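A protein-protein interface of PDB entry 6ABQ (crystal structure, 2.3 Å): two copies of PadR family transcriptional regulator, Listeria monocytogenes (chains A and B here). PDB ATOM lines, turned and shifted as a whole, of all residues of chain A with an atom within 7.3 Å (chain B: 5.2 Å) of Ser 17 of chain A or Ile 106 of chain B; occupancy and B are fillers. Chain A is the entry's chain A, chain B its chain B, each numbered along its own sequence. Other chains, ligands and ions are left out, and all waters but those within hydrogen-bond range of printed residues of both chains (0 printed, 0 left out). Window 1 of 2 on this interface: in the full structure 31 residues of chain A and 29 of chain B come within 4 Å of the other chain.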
ATOM      1  N   LEU A  13     -22.139 -13.358   3.056  1.00  0.00           N
ATOM      2  CA  LEU A  13     -21.352 -14.042   2.016  1.00  0.00           C
ATOM      3  C   LEU A  13     -21.345 -15.562   2.106  1.00  0.00           C
ATOM      4  O   LEU A  13     -21.124 -16.237   1.101  1.00  0.00           O
ATOM      5  CB  LEU A  13     -19.905 -13.533   2.013  1.00  0.00           C
ATOM      6  CG  LEU A  13     -19.477 -12.500   0.970  1.00  0.00           C
ATOM      7  CD1 LEU A  13     -20.120 -11.142   1.212  1.00  0.00           C
ATOM      8  CD2 LEU A  13     -17.961 -12.376   0.928  1.00  0.00           C
ATOM      9  N   LEU A  14     -21.583 -16.082   3.311  1.00  0.00           N
ATOM     10  CA  LEU A  14     -21.597 -17.521   3.580  1.00  0.00           C
ATOM     11  C   LEU A  14     -22.929 -18.220   3.276  1.00  0.00           C
ATOM     12  O   LEU A  14     -23.014 -19.451   3.365  1.00  0.00           O
ATOM     13  CB  LEU A  14     -21.177 -17.794   5.031  1.00  0.00           C
ATOM     14  CG  LEU A  14     -19.703 -17.637   5.415  1.00  0.00           C
ATOM     15  CD1 LEU A  14     -19.557 -17.717   6.929  1.00  0.00           C
ATOM     16  CD2 LEU A  14     -18.801 -18.660   4.731  1.00  0.00           C
ATOM     17  N   LYS A  15     -23.960 -17.443   2.935  1.00  0.00           N
ATOM     18  CA  LYS A  15     -25.256 -17.989   2.520  1.00  0.00           C
ATOM     19  C   LYS A  15     -25.094 -18.820   1.252  1.00  0.00           C
ATOM     20  O   LYS A  15     -24.541 -18.348   0.252  1.00  0.00           O
ATOM     21  CB  LYS A  15     -26.281 -16.873   2.283  1.00  0.00           C
ATOM     22  CG  LYS A  15     -26.778 -16.178   3.539  1.00  0.00           C
ATOM     23  CD  LYS A  15     -27.877 -16.960   4.253  1.00  0.00           C
ATOM     24  CE  LYS A  15     -28.397 -16.179   5.456  1.00  0.00           C
ATOM     25  NZ  LYS A  15     -29.375 -16.957   6.267  1.00  0.00           N
ATOM     26  N   GLY A  16     -25.567 -20.063   1.307  1.00  0.00           N
ATOM     27  CA  GLY A  16     -25.389 -21.009   0.196  1.00  0.00           C
ATOM     28  C   GLY A  16     -24.180 -21.903   0.391  1.00  0.00           C
ATOM     29  O   GLY A  16     -24.219 -23.100   0.057  1.00  0.00           O
ATOM     30  N   SER A  17     -23.107 -21.327   0.931  1.00  0.00           N
ATOM     31  CA  SER A  17     -21.889 -22.077   1.240  1.00  0.00           C
ATOM     32  C   SER A  17     -22.025 -22.854   2.540  1.00  0.00           C
ATOM     33  O   SER A  17     -21.528 -23.971   2.641  1.00  0.00           O
ATOM     34  CB  SER A  17     -20.675 -21.152   1.300  1.00  0.00           C
ATOM     35  OG  SER A  17     -20.308 -20.750  -0.001  1.00  0.00           O
ATOM     36  N   LEU A  18     -22.714 -22.247   3.512  1.00  0.00           N
ATOM     37  CA  LEU A  18     -22.903 -22.805   4.855  1.00  0.00           C
ATOM     38  C   LEU A  18     -23.508 -24.201   4.884  1.00  0.00           C
ATOM     39  O   LEU A  18     -22.977 -25.081   5.566  1.00  0.00           O
ATOM     40  CB  LEU A  18     -23.714 -21.857   5.747  1.00  0.00           C
ATOM     41  CG  LEU A  18     -22.915 -20.846   6.572  1.00  0.00           C
ATOM     42  CD1 LEU A  18     -23.861 -20.028   7.448  1.00  0.00           C
ATOM     43  CD2 LEU A  18     -21.838 -21.529   7.413  1.00  0.00           C
ATOM     44  N   GLU A  19     -24.597 -24.391   4.137  1.00  0.00           N
ATOM     45  CA  GLU A  19     -25.243 -25.690   3.999  1.00  0.00           C
ATOM     46  C   GLU A  19     -24.277 -26.772   3.477  1.00  0.00           C
ATOM     47  O   GLU A  19     -24.244 -27.886   4.008  1.00  0.00           O
ATOM     48  CB  GLU A  19     -26.463 -25.576   3.087  1.00  0.00           C
ATOM     49  CG  GLU A  19     -27.325 -26.821   3.083  1.00  0.00           C
ATOM     50  CD  GLU A  19     -28.577 -26.688   2.249  1.00  0.00           C
ATOM     51  OE1 GLU A  19     -29.421 -25.816   2.554  1.00  0.00           O
ATOM     52  OE2 GLU A  19     -28.725 -27.485   1.299  1.00  0.00           O
ATOM     53  N   GLY A  20     -23.495 -26.421   2.455  1.00  0.00           N
ATOM     54  CA  GLY A  20     -22.531 -27.323   1.833  1.00  0.00           C
ATOM     55  C   GLY A  20     -21.433 -27.751   2.786  1.00  0.00           C
ATOM     56  O   GLY A  20     -21.051 -28.926   2.811  1.00  0.00           O
ATOM     57  N   MET A  21     -20.939 -26.788   3.567  1.00  0.00           N
ATOM     58  CA  MET A  21     -19.918 -27.027   4.593  1.00  0.00           C
ATOM     59  C   MET A  21     -20.395 -28.017   5.646  1.00  0.00           C
ATOM     60  O   MET A  21     -19.663 -28.946   6.002  1.00  0.00           O
ATOM     61  CB  MET A  21     -19.472 -25.713   5.256  1.00  0.00           C
ATOM     62  CG  MET A  21     -18.725 -24.732   4.358  1.00  0.00           C
ATOM     63  SD  MET A  21     -17.211 -25.414   3.662  1.00  0.00           S
ATOM     64  CE  MET A  21     -17.810 -26.143   2.141  1.00  0.00           C
ATOM     65  N   ILE A  22     -21.628 -27.817   6.109  1.00  0.00           N
ATOM     66  CA  ILE A  22     -22.236 -28.650   7.143  1.00  0.00           C
ATOM     67  C   ILE A  22     -22.432 -30.084   6.634  1.00  0.00           C
ATOM     68  O   ILE A  22     -22.024 -31.029   7.307  1.00  0.00           O
ATOM     69  CB  ILE A  22     -23.531 -28.005   7.708  1.00  0.00           C
ATOM     70  CG1 ILE A  22     -23.173 -26.684   8.412  1.00  0.00           C
ATOM     71  CG2 ILE A  22     -24.232 -28.955   8.678  1.00  0.00           C
ATOM     72  CD1 ILE A  22     -24.335 -25.794   8.798  1.00  0.00           C
ATOM     73  N   LEU A  23     -23.011 -30.228   5.438  1.00  0.00           N
ATOM     74  CA  LEU A  23     -23.127 -31.524   4.769  1.00  0.00           C
ATOM     75  C   LEU A  23     -21.762 -32.223   4.628  1.00  0.00           C
ATOM     76  O   LEU A  23     -21.653 -33.423   4.906  1.00  0.00           O
ATOM     77  CB  LEU A  23     -23.825 -31.394   3.397  1.00  0.00           C
ATOM     78  CG  LEU A  23     -25.328 -31.062   3.314  1.00  0.00           C
ATOM     79  CD1 LEU A  23     -25.729 -30.728   1.884  1.00  0.00           C
ATOM     80  CD2 LEU A  23     -26.213 -32.172   3.857  1.00  0.00           C
ATOM     81  N   LEU A  40     -16.852 -25.201  12.309  1.00  0.00           N
ATOM     82  CA  LEU A  40     -16.936 -24.033  11.428  1.00  0.00           C
ATOM     83  C   LEU A  40     -16.204 -22.807  11.993  1.00  0.00           C
ATOM     84  O   LEU A  40     -15.567 -22.078  11.233  1.00  0.00           O
ATOM     85  CB  LEU A  40     -18.396 -23.697  11.076  1.00  0.00           C
ATOM     86  CG  LEU A  40     -19.166 -24.766  10.287  1.00  0.00           C
ATOM     87  CD1 LEU A  40     -20.670 -24.554  10.395  1.00  0.00           C
ATOM     88  CD2 LEU A  40     -18.715 -24.821   8.831  1.00  0.00           C
ATOM     89  N   LEU A  43     -12.418 -23.399  11.677  1.00  0.00           N
ATOM     90  CA  LEU A  43     -12.105 -23.228  10.260  1.00  0.00           C
ATOM     91  C   LEU A  43     -11.848 -21.758   9.900  1.00  0.00           C
ATOM     92  O   LEU A  43     -11.195 -21.466   8.904  1.00  0.00           O
ATOM     93  CB  LEU A  43     -13.263 -23.787   9.424  1.00  0.00           C
ATOM     94  CG  LEU A  43     -13.231 -23.887   7.898  1.00  0.00           C
ATOM     95  CD1 LEU A  43     -12.102 -24.797   7.444  1.00  0.00           C
ATOM     96  CD2 LEU A  43     -14.573 -24.409   7.413  1.00  0.00           C
ATOM     97  N   PHE A  45     -14.650 -19.406  10.399  1.00  0.00           N
ATOM     98  CA  PHE A  45     -15.964 -18.768  10.344  1.00  0.00           C
ATOM     99  C   PHE A  45     -16.459 -18.531  11.773  1.00  0.00           C
ATOM    100  O   PHE A  45     -17.291 -19.273  12.312  1.00  0.00           O
ATOM    101  CB  PHE A  45     -16.943 -19.556   9.459  1.00  0.00           C
ATOM    102  CG  PHE A  45     -16.433 -19.830   8.054  1.00  0.00           C
ATOM    103  CD1 PHE A  45     -15.724 -18.856   7.328  1.00  0.00           C
ATOM    104  CD2 PHE A  45     -16.688 -21.063   7.440  1.00  0.00           C
ATOM    105  CE1 PHE A  45     -15.257 -19.114   6.045  1.00  0.00           C
ATOM    106  CE2 PHE A  45     -16.232 -21.321   6.150  1.00  0.00           C
ATOM    107  CZ  PHE A  45     -15.512 -20.347   5.454  1.00  0.00           C
ATOM    108  N   ARG A  59     -33.490 -27.528   8.331  1.00  0.00           N
ATOM    109  CA  ARG A  59     -33.650 -27.414   6.878  1.00  0.00           C
ATOM    110  C   ARG A  59     -33.189 -28.685   6.150  1.00  0.00           C
ATOM    111  O   ARG A  59     -33.880 -29.170   5.247  1.00  0.00           O
ATOM    112  CB  ARG A  59     -32.933 -26.174   6.335  1.00  0.00           C
ATOM    113  CG  ARG A  59     -33.165 -25.947   4.848  1.00  0.00           C
ATOM    114  CD  ARG A  59     -32.710 -24.568   4.410  1.00  0.00           C
ATOM    115  NE  ARG A  59     -31.282 -24.516   4.095  1.00  0.00           N
ATOM    116  CZ  ARG A  59     -30.408 -23.645   4.607  1.00  0.00           C
ATOM    117  NH1 ARG A  59     -30.783 -22.727   5.487  1.00  0.00           N
ATOM    118  NH2 ARG A  59     -29.138 -23.697   4.224  1.00  0.00           N
ATOM    119  N   PHE A  95     -23.628 -29.858  -4.669  1.00  0.00           N
ATOM    120  CA  PHE A  95     -23.111 -28.608  -4.089  1.00  0.00           C
ATOM    121  C   PHE A  95     -21.721 -28.244  -4.612  1.00  0.00           C
ATOM    122  O   PHE A  95     -21.498 -27.094  -5.002  1.00  0.00           O
ATOM    123  CB  PHE A  95     -23.097 -28.633  -2.550  1.00  0.00           C
ATOM    124  CG  PHE A  95     -22.218 -27.570  -1.937  1.00  0.00           C
ATOM    125  CD1 PHE A  95     -22.659 -26.245  -1.843  1.00  0.00           C
ATOM    126  CD2 PHE A  95     -20.931 -27.878  -1.485  1.00  0.00           C
ATOM    127  CE1 PHE A  95     -21.842 -25.257  -1.301  1.00  0.00           C
ATOM    128  CE2 PHE A  95     -20.110 -26.892  -0.942  1.00  0.00           C
ATOM    129  CZ  PHE A  95     -20.569 -25.583  -0.846  1.00  0.00           C
ATOM    130  N   TRP A  96     -20.801 -29.217  -4.596  1.00  0.00           N
ATOM    131  CA  TRP A  96     -19.423 -29.012  -5.065  1.00  0.00           C
ATOM    132  C   TRP A  96     -19.346 -28.661  -6.559  1.00  0.00           C
ATOM    133  O   TRP A  96     -18.532 -27.820  -6.960  1.00  0.00           O
ATOM    134  CB  TRP A  96     -18.530 -30.219  -4.730  1.00  0.00           C
ATOM    135  CG  TRP A  96     -18.210 -30.356  -3.250  1.00  0.00           C
ATOM    136  CD1 TRP A  96     -18.541 -31.401  -2.434  1.00  0.00           C
ATOM    137  CD2 TRP A  96     -17.515 -29.407  -2.420  1.00  0.00           C
ATOM    138  NE1 TRP A  96     -18.093 -31.170  -1.152  1.00  0.00           N
ATOM    139  CE2 TRP A  96     -17.461 -29.955  -1.115  1.00  0.00           C
ATOM    140  CE3 TRP A  96     -16.933 -28.148  -2.653  1.00  0.00           C
ATOM    141  CZ2 TRP A  96     -16.842 -29.291  -0.048  1.00  0.00           C
ATOM    142  CZ3 TRP A  96     -16.321 -27.487  -1.595  1.00  0.00           C
ATOM    143  CH2 TRP A  96     -16.276 -28.063  -0.308  1.00  0.00           C
ATOM    144  N   TRP A  99     -20.791 -24.995  -6.650  1.00  0.00           N
ATOM    145  CA  TRP A  99     -19.784 -24.141  -6.018  1.00  0.00           C
ATOM    146  C   TRP A  99     -18.553 -23.927  -6.908  1.00  0.00           C
ATOM    147  O   TRP A  99     -18.023 -22.823  -6.949  1.00  0.00           O
ATOM    148  CB  TRP A  99     -19.372 -24.670  -4.631  1.00  0.00           C
ATOM    149  CG  TRP A  99     -18.509 -23.681  -3.881  1.00  0.00           C
ATOM    150  CD1 TRP A  99     -18.937 -22.644  -3.095  1.00  0.00           C
ATOM    151  CD2 TRP A  99     -17.077 -23.617  -3.883  1.00  0.00           C
ATOM    152  NE1 TRP A  99     -17.860 -21.946  -2.595  1.00  0.00           N
ATOM    153  CE2 TRP A  99     -16.705 -22.519  -3.060  1.00  0.00           C
ATOM    154  CE3 TRP A  99     -16.067 -24.388  -4.486  1.00  0.00           C
ATOM    155  CZ2 TRP A  99     -15.361 -22.169  -2.833  1.00  0.00           C
ATOM    156  CZ3 TRP A  99     -14.728 -24.039  -4.261  1.00  0.00           C
ATOM    157  CH2 TRP A  99     -14.389 -22.941  -3.435  1.00  0.00           C
ATOM    158  N   ILE A 102     -19.670 -21.567  -9.757  1.00  0.00           N
ATOM    159  CA  ILE A 102     -19.830 -20.212  -9.235  1.00  0.00           C
ATOM    160  C   ILE A 102     -18.492 -19.506  -8.984  1.00  0.00           C
ATOM    161  O   ILE A 102     -18.359 -18.321  -9.317  1.00  0.00           O
ATOM    162  CB  ILE A 102     -20.809 -20.193  -8.030  1.00  0.00           C
ATOM    163  CG1 ILE A 102     -22.232 -19.965  -8.546  1.00  0.00           C
ATOM    164  CG2 ILE A 102     -20.475 -19.113  -7.007  1.00  0.00           C
ATOM    165  CD1 ILE A 102     -23.294 -20.775  -7.831  1.00  0.00           C
ATOM    166  N   LEU B  13     -26.667 -20.291  -3.601  1.00  0.00           N
ATOM    167  CA  LEU B  13     -25.248 -19.932  -3.573  1.00  0.00           C
ATOM    168  C   LEU B  13     -24.994 -18.485  -3.992  1.00  0.00           C
ATOM    169  O   LEU B  13     -24.107 -17.833  -3.439  1.00  0.00           O
ATOM    170  CB  LEU B  13     -24.432 -20.882  -4.447  1.00  0.00           C
ATOM    171  CG  LEU B  13     -23.683 -22.043  -3.789  1.00  0.00           C
ATOM    172  CD1 LEU B  13     -23.393 -23.122  -4.824  1.00  0.00           C
ATOM    173  CD2 LEU B  13     -22.390 -21.567  -3.128  1.00  0.00           C
ATOM    174  N   ILE B 102     -12.788 -16.578   2.360  1.00  0.00           N
ATOM    175  CA  ILE B 102     -13.784 -17.664   2.333  1.00  0.00           C
ATOM    176  C   ILE B 102     -13.424 -18.730   1.282  1.00  0.00           C
ATOM    177  O   ILE B 102     -13.411 -19.921   1.604  1.00  0.00           O
ATOM    178  CB  ILE B 102     -15.243 -17.144   2.148  1.00  0.00           C
ATOM    179  CG1 ILE B 102     -15.665 -16.259   3.326  1.00  0.00           C
ATOM    180  CG2 ILE B 102     -16.225 -18.304   2.045  1.00  0.00           C
ATOM    181  CD1 ILE B 102     -16.821 -15.321   3.022  1.00  0.00           C
ATOM    182  N   GLN B 103     -13.128 -18.289   0.054  1.00  0.00           N
ATOM    183  CA  GLN B 103     -12.677 -19.169  -1.038  1.00  0.00           C
ATOM    184  C   GLN B 103     -11.477 -20.027  -0.620  1.00  0.00           C
ATOM    185  O   GLN B 103     -11.486 -21.223  -0.854  1.00  0.00           O
ATOM    186  CB  GLN B 103     -12.356 -18.363  -2.310  1.00  0.00           C
ATOM    187  CG  GLN B 103     -11.604 -19.133  -3.407  1.00  0.00           C
ATOM    188  CD  GLN B 103     -11.090 -18.245  -4.537  1.00  0.00           C
ATOM    189  OE1 GLN B 103     -11.455 -18.440  -5.694  1.00  0.00           O
ATOM    190  NE2 GLN B 103     -10.233 -17.270  -4.208  1.00  0.00           N
ATOM    191  N   GLY B 104     -10.476 -19.407   0.010  1.00  0.00           N
ATOM    192  CA  GLY B 104      -9.286 -20.108   0.516  1.00  0.00           C
ATOM    193  C   GLY B 104      -9.624 -21.233   1.481  1.00  0.00           C
ATOM    194  O   GLY B 104      -9.130 -22.353   1.334  1.00  0.00           O
ATOM    195  N   LYS B 105     -10.492 -20.931   2.447  1.00  0.00           N
ATOM    196  CA  LYS B 105     -10.928 -21.896   3.455  1.00  0.00           C
ATOM    197  C   LYS B 105     -11.767 -23.054   2.889  1.00  0.00           C
ATOM    198  O   LYS B 105     -11.532 -24.203   3.247  1.00  0.00           O
ATOM    199  CB  LYS B 105     -11.658 -21.193   4.613  1.00  0.00           C
ATOM    200  CG  LYS B 105     -10.798 -20.238   5.438  1.00  0.00           C
ATOM    201  CD  LYS B 105      -9.620 -20.934   6.120  1.00  0.00           C
ATOM    202  CE  LYS B 105      -8.847 -19.963   6.999  1.00  0.00           C
ATOM    203  NZ  LYS B 105      -7.895 -20.653   7.917  1.00  0.00           N
ATOM    204  N   ILE B 106     -12.723 -22.751   2.006  1.00  0.00           N
ATOM    205  CA  ILE B 106     -13.572 -23.784   1.370  1.00  0.00           C
ATOM    206  C   ILE B 106     -12.748 -24.698   0.439  1.00  0.00           C
ATOM    207  O   ILE B 106     -13.014 -25.906   0.343  1.00  0.00           O
ATOM    208  CB  ILE B 106     -14.801 -23.175   0.635  1.00  0.00           C
ATOM    209  CG1 ILE B 106     -15.698 -22.398   1.615  1.00  0.00           C
ATOM    210  CG2 ILE B 106     -15.621 -24.260  -0.060  1.00  0.00           C
ATOM    211  CD1 ILE B 106     -16.893 -21.715   0.976  1.00  0.00           C
ATOM    212  N   MET B 107     -11.740 -24.119  -0.219  1.00  0.00           N
ATOM    213  CA  MET B 107     -10.826 -24.891  -1.067  1.00  0.00           C
ATOM    214  C   MET B 107      -9.999 -25.906  -0.284  1.00  0.00           C
ATOM    215  O   MET B 107      -9.738 -27.003  -0.782  1.00  0.00           O
ATOM    216  CB  MET B 107      -9.937 -23.983  -1.919  1.00  0.00           C
ATOM    217  CG  MET B 107     -10.677 -23.301  -3.065  1.00  0.00           C
ATOM    218  SD  MET B 107     -10.785 -24.197  -4.632  1.00  0.00           S
ATOM    219  CE  MET B 107     -11.565 -25.749  -4.233  1.00  0.00           C
ATOM    220  N   GLN B 108      -9.600 -25.541   0.934  1.00  0.00           N
ATOM    221  CA  GLN B 108      -8.943 -26.474   1.850  1.00  0.00           C
ATOM    222  C   GLN B 108      -9.882 -27.615   2.244  1.00  0.00           C
ATOM    223  O   GLN B 108      -9.464 -28.773   2.296  1.00  0.00           O
ATOM    224  CB  GLN B 108      -8.444 -25.750   3.097  1.00  0.00           C
ATOM    225  CG  GLN B 108      -7.195 -24.914   2.884  1.00  0.00           C
ATOM    226  CD  GLN B 108      -6.760 -24.228   4.159  1.00  0.00           C
ATOM    227  OE1 GLN B 108      -7.043 -23.046   4.372  1.00  0.00           O
ATOM    228  NE2 GLN B 108      -6.089 -24.974   5.034  1.00  0.00           N
ATOM    229  N   VAL B 109     -11.147 -27.270   2.507  1.00  0.00           N
ATOM    230  CA  VAL B 109     -12.209 -28.229   2.813  1.00  0.00           C
ATOM    231  C   VAL B 109     -12.422 -29.195   1.636  1.00  0.00           C
ATOM    232  O   VAL B 109     -12.417 -30.411   1.835  1.00  0.00           O
ATOM    233  CB  VAL B 109     -13.524 -27.508   3.227  1.00  0.00           C
ATOM    234  CG1 VAL B 109     -14.711 -28.463   3.258  1.00  0.00           C
ATOM    235  CG2 VAL B 109     -13.368 -26.831   4.582  1.00  0.00           C
ATOM    236  N   LYS B 110     -12.579 -28.648   0.424  1.00  0.00           N
ATOM    237  CA  LYS B 110     -12.757 -29.441  -0.802  1.00  0.00           C
ATOM    238  C   LYS B 110     -11.583 -30.393  -1.066  1.00  0.00           C
ATOM    239  O   LYS B 110     -11.791 -31.534  -1.472  1.00  0.00           O
ATOM    240  CB  LYS B 110     -12.995 -28.535  -2.020  1.00  0.00           C
ATOM    241  CG  LYS B 110     -13.385 -29.273  -3.301  1.00  0.00           C
ATOM    242  CD  LYS B 110     -13.744 -28.294  -4.413  1.00  0.00           C
ATOM    243  CE  LYS B 110     -13.242 -28.752  -5.775  1.00  0.00           C
ATOM    244  NZ  LYS B 110     -14.203 -29.645  -6.480  1.00  0.00           N
ATOM    245  N   GLY B 111     -10.364 -29.916  -0.827  1.00  0.00           N
ATOM    246  CA  GLY B 111      -9.152 -30.723  -1.030  1.00  0.00           C
ATOM    247  C   GLY B 111      -8.907 -31.779   0.042  1.00  0.00           C
ATOM    248  O   GLY B 111      -7.988 -32.591  -0.086  1.00  0.00           O
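The backbone NH of Phe 45 of chain A is in hydrogen-bond range of the backbone carbonyl oxygen of Leu 40 of chain A, at 2.9 Å.
Ile 102 of chain B touches Leu 14 of chain A (CG2 to CD2, 3.7 Å). Ser 17 of chain A touches Ile 106 of chain B. CE of Met 21 of chain A touches CG2 of Ile 106 of chain B, at 3.6 Å. Met 21 of chain A touches Val 109 of chain B. Lys 105 of chain B touches Leu 43 of chain A. Ile 102 of chain B touches Phe 45 of chain A (CG1 to CE1, 3.96 Å). CZ3 of Trp 96 of chain A touches CG2 of Ile 106 of chain B, at 3.6 Å. Trp 99 of chain A touches Ile 106 of chain B. Trp 99 of chain A touches Met 107 of chain B (CZ3 to CE, 3.6 Å). CD1 of Ile 102 of chain A touches CB of Leu 13 of chain B (3.6 Å).
Ser 17 of chain A touches two residues of chain B. Of the printed residues of chain B, Met 21 of chain A touches Ile 106 and Val 109. Of the printed residues of chain B, Phe 45 of chain A touches Ile 102 (3.96 Å). The nearest printed residue of chain B that does not touch Ser 17 of chain A is Ile 102 of chain B (5.2 Å). The nearest residue of chain A that does not touch Ile 106 of chain B is Phe 45 of chain A (4.4 Å).
Of the 11 printed residues of chain B, 7 touch a printed residue of chain A. Printed residues of chain B that touch a printed residue of chain A: Leu 13, Ile 102, Lys 105, Ile 106, Met 107, Val 109 and Lys 110. Among the printed residues, 18 pairs touch across the chains. Among the printed residues, no Asp or Glu carboxylate lies within 4 Å of a Lys or Arg side-chain nitrogen of the other chain.
Leu 13 of chain A touches Ile 102 of chain B, and with the chains exchanged Ile 102 of chain A touches Leu 13 of chain B. Of the 18 pairs that touch across the chains among the printed residues, 2 have their exchanged pair printed and touching as well.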
